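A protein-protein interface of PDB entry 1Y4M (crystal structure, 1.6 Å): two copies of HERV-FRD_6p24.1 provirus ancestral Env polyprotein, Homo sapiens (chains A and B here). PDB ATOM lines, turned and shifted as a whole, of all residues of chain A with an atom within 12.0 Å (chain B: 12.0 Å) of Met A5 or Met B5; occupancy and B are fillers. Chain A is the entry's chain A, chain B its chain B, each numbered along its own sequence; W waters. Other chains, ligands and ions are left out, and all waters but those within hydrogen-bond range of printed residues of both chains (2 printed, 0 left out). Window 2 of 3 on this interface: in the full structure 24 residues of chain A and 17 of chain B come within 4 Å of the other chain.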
ATOM      1  N   ASN A   1      23.867 -12.892  44.347  1.00  0.00           N
ATOM      2  CA  ASN A   1      25.293 -13.267  44.416  1.00  0.00           C
ATOM      3  C   ASN A   1      25.533 -14.743  44.126  1.00  0.00           C
ATOM      4  O   ASN A   1      26.669 -15.186  44.124  1.00  0.00           O
ATOM      5  CB  ASN A   1      25.848 -12.873  45.786  1.00  0.00           C
ATOM      6  CG  ASN A   1      26.087 -11.380  45.921  1.00  0.00           C
ATOM      7  OD1 ASN A   1      25.196 -10.549  45.668  1.00  0.00           O
ATOM      8  ND2 ASN A   1      27.284 -11.031  46.365  1.00  0.00           N
ATOM      9  N   ILE A   2      24.467 -15.514  43.937  1.00  0.00           N
ATOM     10  CA  ILE A   2      24.629 -16.920  43.573  1.00  0.00           C
ATOM     11  C   ILE A   2      24.183 -17.138  42.156  1.00  0.00           C
ATOM     12  O   ILE A   2      23.675 -16.220  41.528  1.00  0.00           O
ATOM     13  N   ASP A   3      24.388 -18.363  41.676  1.00  0.00           N
ATOM     14  CA  ASP A   3      24.013 -18.777  40.325  1.00  0.00           C
ATOM     15  C   ASP A   3      23.902 -17.688  39.251  1.00  0.00           C
ATOM     16  O   ASP A   3      22.796 -17.333  38.835  1.00  0.00           O
ATOM     17  N   THR A   4      25.040 -17.166  38.801  1.00  0.00           N
ATOM     18  CA  THR A   4      25.046 -16.166  37.738  1.00  0.00           C
ATOM     19  C   THR A   4      25.175 -16.958  36.448  1.00  0.00           C
ATOM     20  O   THR A   4      24.675 -16.557  35.402  1.00  0.00           O
ATOM     21  N   MET A   5      25.859 -18.093  36.556  1.00  0.00           N
ATOM     22  CA  MET A   5      26.095 -19.003  35.440  1.00  0.00           C
ATOM     23  C   MET A   5      24.806 -19.360  34.710  1.00  0.00           C
ATOM     24  O   MET A   5      24.637 -19.030  33.537  1.00  0.00           O
ATOM     25  CB  MET A   5      26.764 -20.283  35.953  1.00  0.00           C
ATOM     26  CG  MET A   5      28.284 -20.292  35.879  1.00  0.00           C
ATOM     27  SD  MET A   5      28.862 -21.142  34.394  1.00  0.00           S
ATOM     28  CE  MET A   5      28.447 -19.935  33.135  1.00  0.00           C
ATOM     29  N   ALA A   6      23.908 -20.045  35.412  1.00  0.00           N
ATOM     30  CA  ALA A   6      22.631 -20.460  34.848  1.00  0.00           C
ATOM     31  C   ALA A   6      21.913 -19.282  34.196  1.00  0.00           C
ATOM     32  O   ALA A   6      21.317 -19.418  33.127  1.00  0.00           O
ATOM     33  CB  ALA A   6      21.759 -21.064  35.939  1.00  0.00           C
ATOM     34  N   LYS A   7      21.972 -18.127  34.849  1.00  0.00           N
ATOM     35  CA  LYS A   7      21.331 -16.930  34.325  1.00  0.00           C
ATOM     36  C   LYS A   7      22.067 -16.409  33.098  1.00  0.00           C
ATOM     37  O   LYS A   7      21.446 -15.970  32.132  1.00  0.00           O
ATOM     38  CB  LYS A   7      21.278 -15.831  35.392  1.00  0.00           C
ATOM     39  CG  LYS A   7      20.779 -14.491  34.862  1.00  0.00           C
ATOM     40  CD  LYS A   7      20.447 -13.514  35.980  1.00  0.00           C
ATOM     41  CE  LYS A   7      21.660 -13.169  36.824  1.00  0.00           C
ATOM     42  NZ  LYS A   7      21.282 -12.247  37.932  1.00  0.00           N
ATOM     43  N   ALA A   8      23.394 -16.458  33.142  1.00  0.00           N
ATOM     44  CA  ALA A   8      24.202 -15.989  32.025  1.00  0.00           C
ATOM     45  C   ALA A   8      23.850 -16.766  30.761  1.00  0.00           C
ATOM     46  O   ALA A   8      23.826 -16.207  29.666  1.00  0.00           O
ATOM     47  CB  ALA A   8      25.681 -16.151  32.345  1.00  0.00           C
ATOM     48  N   LEU A   9      23.574 -18.055  30.922  1.00  0.00           N
ATOM     49  CA  LEU A   9      23.217 -18.906  29.793  1.00  0.00           C
ATOM     50  C   LEU A   9      21.957 -18.393  29.122  1.00  0.00           C
ATOM     51  O   LEU A   9      21.887 -18.312  27.895  1.00  0.00           O
ATOM     52  CB  LEU A   9      22.984 -20.339  30.261  1.00  0.00           C
ATOM     53  CG  LEU A   9      24.194 -21.093  30.806  1.00  0.00           C
ATOM     54  CD1 LEU A   9      23.742 -22.411  31.400  1.00  0.00           C
ATOM     55  CD2 LEU A   9      25.201 -21.317  29.688  1.00  0.00           C
ATOM     56  N   THR A  10      20.955 -18.054  29.924  1.00  0.00           N
ATOM     57  CA  THR A  10      19.703 -17.556  29.370  1.00  0.00           C
ATOM     58  C   THR A  10      19.928 -16.222  28.684  1.00  0.00           C
ATOM     59  O   THR A  10      19.429 -15.980  27.585  1.00  0.00           O
ATOM     60  CB  THR A  10      18.638 -17.380  30.464  1.00  0.00           C
ATOM     61  OG1 THR A  10      18.368 -18.650  31.070  1.00  0.00           O
ATOM     62  CG2 THR A  10      17.353 -16.837  29.867  1.00  0.00           C
ATOM     63  N   THR A  11      20.689 -15.355  29.337  1.00  0.00           N
ATOM     64  CA  THR A  11      20.985 -14.049  28.783  1.00  0.00           C
ATOM     65  C   THR A  11      21.674 -14.214  27.439  1.00  0.00           C
ATOM     66  O   THR A  11      21.315 -13.561  26.462  1.00  0.00           O
ATOM     67  CB  THR A  11      21.899 -13.266  29.725  1.00  0.00           C
ATOM     68  OG1 THR A  11      21.198 -13.013  30.948  1.00  0.00           O
ATOM     69  CG2 THR A  11      22.321 -11.951  29.096  1.00  0.00           C
ATOM     70  N   MET A  12      22.660 -15.102  27.400  1.00  0.00           N
ATOM     71  CA  MET A  12      23.402 -15.349  26.174  1.00  0.00           C
ATOM     72  C   MET A  12      22.498 -15.895  25.083  1.00  0.00           C
ATOM     73  O   MET A  12      22.599 -15.497  23.921  1.00  0.00           O
ATOM     74  CB  MET A  12      24.536 -16.337  26.428  1.00  0.00           C
ATOM     75  CG  MET A  12      25.384 -16.589  25.204  1.00  0.00           C
ATOM     76  SD  MET A  12      26.817 -17.585  25.570  1.00  0.00           S
ATOM     77  CE  MET A  12      27.957 -16.331  26.112  1.00  0.00           C
ATOM     78  N   GLN A  13      21.620 -16.818  25.457  1.00  0.00           N
ATOM     79  CA  GLN A  13      20.710 -17.401  24.489  1.00  0.00           C
ATOM     80  C   GLN A  13      19.842 -16.327  23.862  1.00  0.00           C
ATOM     81  O   GLN A  13      19.602 -16.339  22.659  1.00  0.00           O
ATOM     82  CB  GLN A  13      19.808 -18.445  25.143  1.00  0.00           C
ATOM     83  CG  GLN A  13      18.830 -19.044  24.157  1.00  0.00           C
ATOM     84  CD  GLN A  13      19.540 -19.748  23.027  1.00  0.00           C
ATOM     85  OE1 GLN A  13      20.161 -20.787  23.228  1.00  0.00           O
ATOM     86  NE2 GLN A  13      19.461 -19.177  21.827  1.00  0.00           N
ATOM     87  N   GLU A  14      19.361 -15.394  24.672  1.00  0.00           N
ATOM     88  CA  GLU A  14      18.521 -14.343  24.130  1.00  0.00           C
ATOM     89  C   GLU A  14      19.365 -13.401  23.281  1.00  0.00           C
ATOM     90  O   GLU A  14      18.884 -12.851  22.293  1.00  0.00           O
ATOM     91  CB  GLU A  14      17.819 -13.594  25.262  1.00  0.00           C
ATOM     92  CG  GLU A  14      17.070 -14.532  26.201  1.00  0.00           C
ATOM     93  CD  GLU A  14      16.093 -13.816  27.103  1.00  0.00           C
ATOM     94  OE1 GLU A  14      16.419 -12.708  27.576  1.00  0.00           O
ATOM     95  OE2 GLU A  14      15.000 -14.375  27.345  1.00  0.00           O
ATOM     96  N   GLN A  15      20.628 -13.228  23.660  1.00  0.00           N
ATOM     97  CA  GLN A  15      21.522 -12.361  22.899  1.00  0.00           C
ATOM     98  C   GLN A  15      21.694 -12.976  21.527  1.00  0.00           C
ATOM     99  O   GLN A  15      21.643 -12.287  20.512  1.00  0.00           O
ATOM    100  CB  GLN A  15      22.890 -12.258  23.569  1.00  0.00           C
ATOM    101  CG  GLN A  15      22.932 -11.351  24.780  1.00  0.00           C
ATOM    102  CD  GLN A  15      24.309 -11.307  25.405  1.00  0.00           C
ATOM    103  OE1 GLN A  15      25.308 -11.111  24.711  1.00  0.00           O
ATOM    104  NE2 GLN A  15      24.374 -11.488  26.720  1.00  0.00           N
ATOM    105  N   ILE A  16      21.906 -14.285  21.508  1.00  0.00           N
ATOM    106  CA  ILE A  16      22.075 -14.990  20.248  1.00  0.00           C
ATOM    107  C   ILE A  16      20.800 -14.888  19.423  1.00  0.00           C
ATOM    108  O   ILE A  16      20.857 -14.655  18.217  1.00  0.00           O
ATOM    109  CB  ILE A  16      22.403 -16.465  20.480  1.00  0.00           C
ATOM    110  CG1 ILE A  16      23.763 -16.591  21.167  1.00  0.00           C
ATOM    111  CG2 ILE A  16      22.401 -17.204  19.157  1.00  0.00           C
ATOM    112  CD1 ILE A  16      24.068 -17.983  21.643  1.00  0.00           C
ATOM    113  N   ASN B   1      19.384 -26.652  35.604  1.00  0.00           N
ATOM    114  CA  ASN B   1      20.023 -27.936  35.870  1.00  0.00           C
ATOM    115  C   ASN B   1      21.431 -27.981  35.281  1.00  0.00           C
ATOM    116  O   ASN B   1      21.706 -27.353  34.260  1.00  0.00           O
ATOM    117  CB  ASN B   1      19.196 -29.075  35.274  1.00  0.00           C
ATOM    118  CG  ASN B   1      19.758 -30.439  35.618  1.00  0.00           C
ATOM    119  OD1 ASN B   1      19.550 -30.951  36.720  1.00  0.00           O
ATOM    120  ND2 ASN B   1      20.490 -31.028  34.679  1.00  0.00           N
ATOM    121  N   ILE B   2      22.312 -28.736  35.927  1.00  0.00           N
ATOM    122  CA  ILE B   2      23.695 -28.865  35.483  1.00  0.00           C
ATOM    123  C   ILE B   2      23.804 -29.410  34.062  1.00  0.00           C
ATOM    124  O   ILE B   2      24.393 -28.771  33.190  1.00  0.00           O
ATOM    125  CB  ILE B   2      24.488 -29.789  36.424  1.00  0.00           C
ATOM    126  CG1 ILE B   2      24.370 -29.286  37.865  1.00  0.00           C
ATOM    127  CG2 ILE B   2      25.948 -29.827  35.999  1.00  0.00           C
ATOM    128  CD1 ILE B   2      24.925 -30.247  38.895  1.00  0.00           C
ATOM    129  N   ASP B   3      23.246 -30.594  33.831  1.00  0.00           N
ATOM    130  CA  ASP B   3      23.293 -31.200  32.506  1.00  0.00           C
ATOM    131  C   ASP B   3      22.642 -30.258  31.498  1.00  0.00           C
ATOM    132  O   ASP B   3      23.081 -30.162  30.352  1.00  0.00           O
ATOM    133  CB  ASP B   3      22.561 -32.547  32.508  1.00  0.00           C
ATOM    134  CG  ASP B   3      22.744 -33.313  31.209  1.00  0.00           C
ATOM    135  OD1 ASP B   3      22.185 -34.424  31.088  1.00  0.00           O
ATOM    136  OD2 ASP B   3      23.449 -32.807  30.310  1.00  0.00           O
ATOM    137  N   THR B   4      21.595 -29.564  31.938  1.00  0.00           N
ATOM    138  CA  THR B   4      20.885 -28.619  31.084  1.00  0.00           C
ATOM    139  C   THR B   4      21.828 -27.482  30.707  1.00  0.00           C
ATOM    140  O   THR B   4      21.865 -27.052  29.555  1.00  0.00           O
ATOM    141  CB  THR B   4      19.650 -28.034  31.801  1.00  0.00           C
ATOM    142  OG1 THR B   4      18.754 -29.095  32.146  1.00  0.00           O
ATOM    143  CG2 THR B   4      18.924 -27.045  30.900  1.00  0.00           C
ATOM    144  N   MET B   5      22.588 -27.002  31.685  1.00  0.00           N
ATOM    145  CA  MET B   5      23.541 -25.929  31.443  1.00  0.00           C
ATOM    146  C   MET B   5      24.550 -26.370  30.390  1.00  0.00           C
ATOM    147  O   MET B   5      24.888 -25.608  29.482  1.00  0.00           O
ATOM    148  CB  MET B   5      24.273 -25.560  32.735  1.00  0.00           C
ATOM    149  CG  MET B   5      23.405 -24.875  33.776  1.00  0.00           C
ATOM    150  SD  MET B   5      24.353 -24.417  35.238  1.00  0.00           S
ATOM    151  CE  MET B   5      25.115 -22.906  34.687  1.00  0.00           C
ATOM    152  N   ALA B   6      25.026 -27.605  30.510  1.00  0.00           N
ATOM    153  CA  ALA B   6      25.993 -28.142  29.559  1.00  0.00           C
ATOM    154  C   ALA B   6      25.380 -28.176  28.166  1.00  0.00           C
ATOM    155  O   ALA B   6      26.013 -27.774  27.188  1.00  0.00           O
ATOM    156  CB  ALA B   6      26.424 -29.541  29.977  1.00  0.00           C
ATOM    157  N   LYS B   7      24.146 -28.662  28.083  1.00  0.00           N
ATOM    158  CA  LYS B   7      23.439 -28.736  26.812  1.00  0.00           C
ATOM    159  C   LYS B   7      23.202 -27.334  26.260  1.00  0.00           C
ATOM    160  O   LYS B   7      23.334 -27.105  25.061  1.00  0.00           O
ATOM    161  CB  LYS B   7      22.103 -29.462  26.990  1.00  0.00           C
ATOM    162  CG  LYS B   7      22.249 -30.945  27.296  1.00  0.00           C
ATOM    163  CD  LYS B   7      20.896 -31.606  27.494  1.00  0.00           C
ATOM    164  CE  LYS B   7      21.035 -33.102  27.729  1.00  0.00           C
ATOM    165  NZ  LYS B   7      21.613 -33.803  26.542  1.00  0.00           N
ATOM    166  N   ALA B   8      22.850 -26.401  27.139  1.00  0.00           N
ATOM    167  CA  ALA B   8      22.612 -25.023  26.723  1.00  0.00           C
ATOM    168  C   ALA B   8      23.883 -24.478  26.091  1.00  0.00           C
ATOM    169  O   ALA B   8      23.848 -23.869  25.026  1.00  0.00           O
ATOM    170  CB  ALA B   8      22.220 -24.172  27.924  1.00  0.00           C
ATOM    171  N   LEU B   9      25.010 -24.703  26.757  1.00  0.00           N
ATOM    172  CA  LEU B   9      26.293 -24.241  26.246  1.00  0.00           C
ATOM    173  C   LEU B   9      26.585 -24.869  24.893  1.00  0.00           C
ATOM    174  O   LEU B   9      27.039 -24.193  23.972  1.00  0.00           O
ATOM    175  CB  LEU B   9      27.413 -24.602  27.220  1.00  0.00           C
ATOM    176  CG  LEU B   9      27.528 -23.785  28.506  1.00  0.00           C
ATOM    177  CD1 LEU B   9      28.482 -24.477  29.469  1.00  0.00           C
ATOM    178  CD2 LEU B   9      28.013 -22.388  28.177  1.00  0.00           C
ATOM    179  N   THR B  10      26.329 -26.167  24.783  1.00  0.00           N
ATOM    180  CA  THR B  10      26.573 -26.897  23.547  1.00  0.00           C
ATOM    181  C   THR B  10      25.776 -26.309  22.396  1.00  0.00           C
ATOM    182  O   THR B  10      26.339 -25.915  21.374  1.00  0.00           O
ATOM    183  CB  THR B  10      26.195 -28.377  23.707  1.00  0.00           C
ATOM    184  OG1 THR B  10      26.963 -28.943  24.774  1.00  0.00           O
ATOM    185  CG2 THR B  10      26.474 -29.150  22.425  1.00  0.00           C
ATOM    186  N   THR B  11      24.462 -26.244  22.566  1.00  0.00           N
ATOM    187  CA  THR B  11      23.616 -25.708  21.517  1.00  0.00           C
ATOM    188  C   THR B  11      23.977 -24.266  21.192  1.00  0.00           C
ATOM    189  O   THR B  11      24.076 -23.899  20.024  1.00  0.00           O
ATOM    190  CB  THR B  11      22.126 -25.769  21.899  1.00  0.00           C
ATOM    191  OG1 THR B  11      21.352 -25.128  20.877  1.00  0.00           O
ATOM    192  CG2 THR B  11      21.883 -25.069  23.228  1.00  0.00           C
ATOM    193  N   MET B  12      24.186 -23.446  22.216  1.00  0.00           N
ATOM    194  CA  MET B  12      24.514 -22.054  21.957  1.00  0.00           C
ATOM    195  C   MET B  12      25.817 -21.916  21.203  1.00  0.00           C
ATOM    196  O   MET B  12      25.988 -20.995  20.408  1.00  0.00           O
ATOM    197  CB  MET B  12      24.576 -21.258  23.257  1.00  0.00           C
ATOM    198  CG  MET B  12      23.222 -21.120  23.920  1.00  0.00           C
ATOM    199  SD  MET B  12      23.214 -19.740  25.036  1.00  0.00           S
ATOM    200  CE  MET B  12      24.229 -20.384  26.353  1.00  0.00           C
ATOM    201  N   GLN B  13      26.741 -22.830  21.459  1.00  0.00           N
ATOM    202  CA  GLN B  13      28.016 -22.795  20.769  1.00  0.00           C
ATOM    203  C   GLN B  13      27.755 -23.102  19.301  1.00  0.00           C
ATOM    204  O   GLN B  13      28.291 -22.446  18.405  1.00  0.00           O
ATOM    205  CB  GLN B  13      28.968 -23.831  21.365  1.00  0.00           C
ATOM    206  CG  GLN B  13      30.255 -23.999  20.582  1.00  0.00           C
ATOM    207  CD  GLN B  13      30.911 -22.668  20.266  1.00  0.00           C
ATOM    208  OE1 GLN B  13      31.259 -21.899  21.166  1.00  0.00           O
ATOM    209  NE2 GLN B  13      31.081 -22.389  18.978  1.00  0.00           N
ATOM    210  N   GLU B  14      26.907 -24.092  19.060  1.00  0.00           N
ATOM    211  CA  GLU B  14      26.570 -24.482  17.701  1.00  0.00           C
ATOM    212  C   GLU B  14      25.795 -23.359  17.019  1.00  0.00           C
ATOM    213  O   GLU B  14      25.931 -23.145  15.817  1.00  0.00           O
ATOM    214  CB  GLU B  14      25.737 -25.763  17.719  1.00  0.00           C
ATOM    215  CG  GLU B  14      26.399 -26.906  18.473  1.00  0.00           C
ATOM    216  CD  GLU B  14      25.498 -28.119  18.610  1.00  0.00           C
ATOM    217  OE1 GLU B  14      24.365 -27.965  19.116  1.00  0.00           O
ATOM    218  OE2 GLU B  14      25.924 -29.227  18.217  1.00  0.00           O
ATOM    219  N   GLN B  15      24.989 -22.640  17.792  1.00  0.00           N
ATOM    220  CA  GLN B  15      24.209 -21.542  17.242  1.00  0.00           C
ATOM    221  C   GLN B  15      25.143 -20.412  16.848  1.00  0.00           C
ATOM    222  O   GLN B  15      24.971 -19.784  15.808  1.00  0.00           O
ATOM    223  CB  GLN B  15      23.209 -21.023  18.274  1.00  0.00           C
ATOM    224  CG  GLN B  15      22.238 -22.067  18.785  1.00  0.00           C
ATOM    225  CD  GLN B  15      21.306 -21.514  19.838  1.00  0.00           C
ATOM    226  OE1 GLN B  15      20.824 -22.245  20.704  1.00  0.00           O
ATOM    227  NE2 GLN B  15      21.040 -20.218  19.767  1.00  0.00           N
ATOM    228  N   ILE B  16      26.129 -20.152  17.696  1.00  0.00           N
ATOM    229  CA  ILE B  16      27.084 -19.092  17.425  1.00  0.00           C
ATOM    230  C   ILE B  16      27.837 -19.357  16.129  1.00  0.00           C
ATOM    231  O   ILE B  16      27.894 -18.499  15.253  1.00  0.00           O
ATOM    232  CB  ILE B  16      28.100 -18.958  18.566  1.00  0.00           C
ATOM    233  CG1 ILE B  16      27.383 -18.467  19.827  1.00  0.00           C
ATOM    234  CG2 ILE B  16      29.210 -17.991  18.169  1.00  0.00           C
ATOM    235  CD1 ILE B  16      28.245 -18.484  21.056  1.00  0.00           C
HETATM  236  O   HOH W   1      20.571 -20.749  27.501  1.00  0.00           O
HETATM  237  O   HOH W   2      20.311 -22.139  25.495  1.00  0.00           O
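No residue of chain B comes within 4 Å of Ile A2. No residue of chain B comes within 4 Å of Asp A3. Ala A6 touches one residue of chain B. No residue of chain B comes within 4 Å of Lys A7. No residue of chain B comes within 4 Å of Ala A8. Of chain B, only Met B5 (3.4 Å), Leu B9 (3.4 Å) and Met B12 (3.5 Å) come within 4 Å of Leu A9. Of the printed residues of chain B, Met A12 touches Met B12. Of the printed residues of chain B, Gln A13 touches Met B12 (3.2 Å) and Gln B15 (2.8 Å). No residue of chain A comes within 4 Å of Asp B3. Of the printed residues of chain A, Met B5 touches Met A5, Ala A6 and Leu A9. Lys B7 touches none of the printed residues of chain A. No residue of chain A comes within 4 Å of Ala B8. Thr B11 touches none of the printed residues of chain A. Of the printed residues of chain A, Gln B15 touches Gln A13 (2.8 Å) and Ile A16 (3.4 Å). Printed residues of chain A within 4 Å of Ile B16: Ile A16 (3.8 Å).
Of the 16 printed residues of chain A, 6 touch a printed residue of chain B. Hydrophobic or aromatic side chains of chain A within 4 Å of the printed part of chain B: Met A5, Leu A9, Met A12 and Ile A16.
The side-chain hydroxyl (OG1) of Thr B11 sits at hydrogen-bond distance from the side-chain amide oxygen (OE1) of Gln B15 (2.9 Å).
Water W2 lies within hydrogen-bond range of OE1 of Gln A13 and SD of Met B12. Water W1 lies within hydrogen-bond range of O of Leu A9 (2.8 Å) and SD of Met B12 (3.8 Å).
Leu A9 touches Met B5, but with the chains exchanged Met A5 does not touch Leu B9 (5.5 Å). Leu A9 touches Met B12, but with the chains exchanged Met A12 does not touch Leu B9 (5.6 Å). Met A12 touches its own counterpart, Met B12. Ile A16 touches Gln B15, but with the chains exchanged Gln A15 does not touch Ile B16 (8.1 Å). 16 positions are printed for both chains. Of the 11 pairs that touch across the chains among the printed residues, 4 have their exchanged pair printed and touching as well.
Met A5 touches Met B5 (CB to CE, 3.3 Å). Ala A6 touches Met B5 (N to CE, 3.2 Å). CD1 of Leu A9 touches CG of Met B5 (3.4 Å). Leu B9 touches Leu A9 (CD2 to CD2, 3.4 Å). Met B12 touches Met A12 (SD to CG, 3.8 Å). Met B12 touches Ile A16 (CB to CD1, 3.7 Å). Ile A16 touches Gln B15. CG1 of Ile B16 touches CD1 of Ile A16 (3.8 Å).
NE2 of Gln A13 sits close to NE2 of Gln B15 (2.8 Å). The backbone carbonyl oxygen (O) of Leu A9 sits close to the side-chain sulfur (SD) of Met B12 (3.5 Å). N of Gln A13 lies within hydrogen-bond range of SD of Met B12 (3.4 Å).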
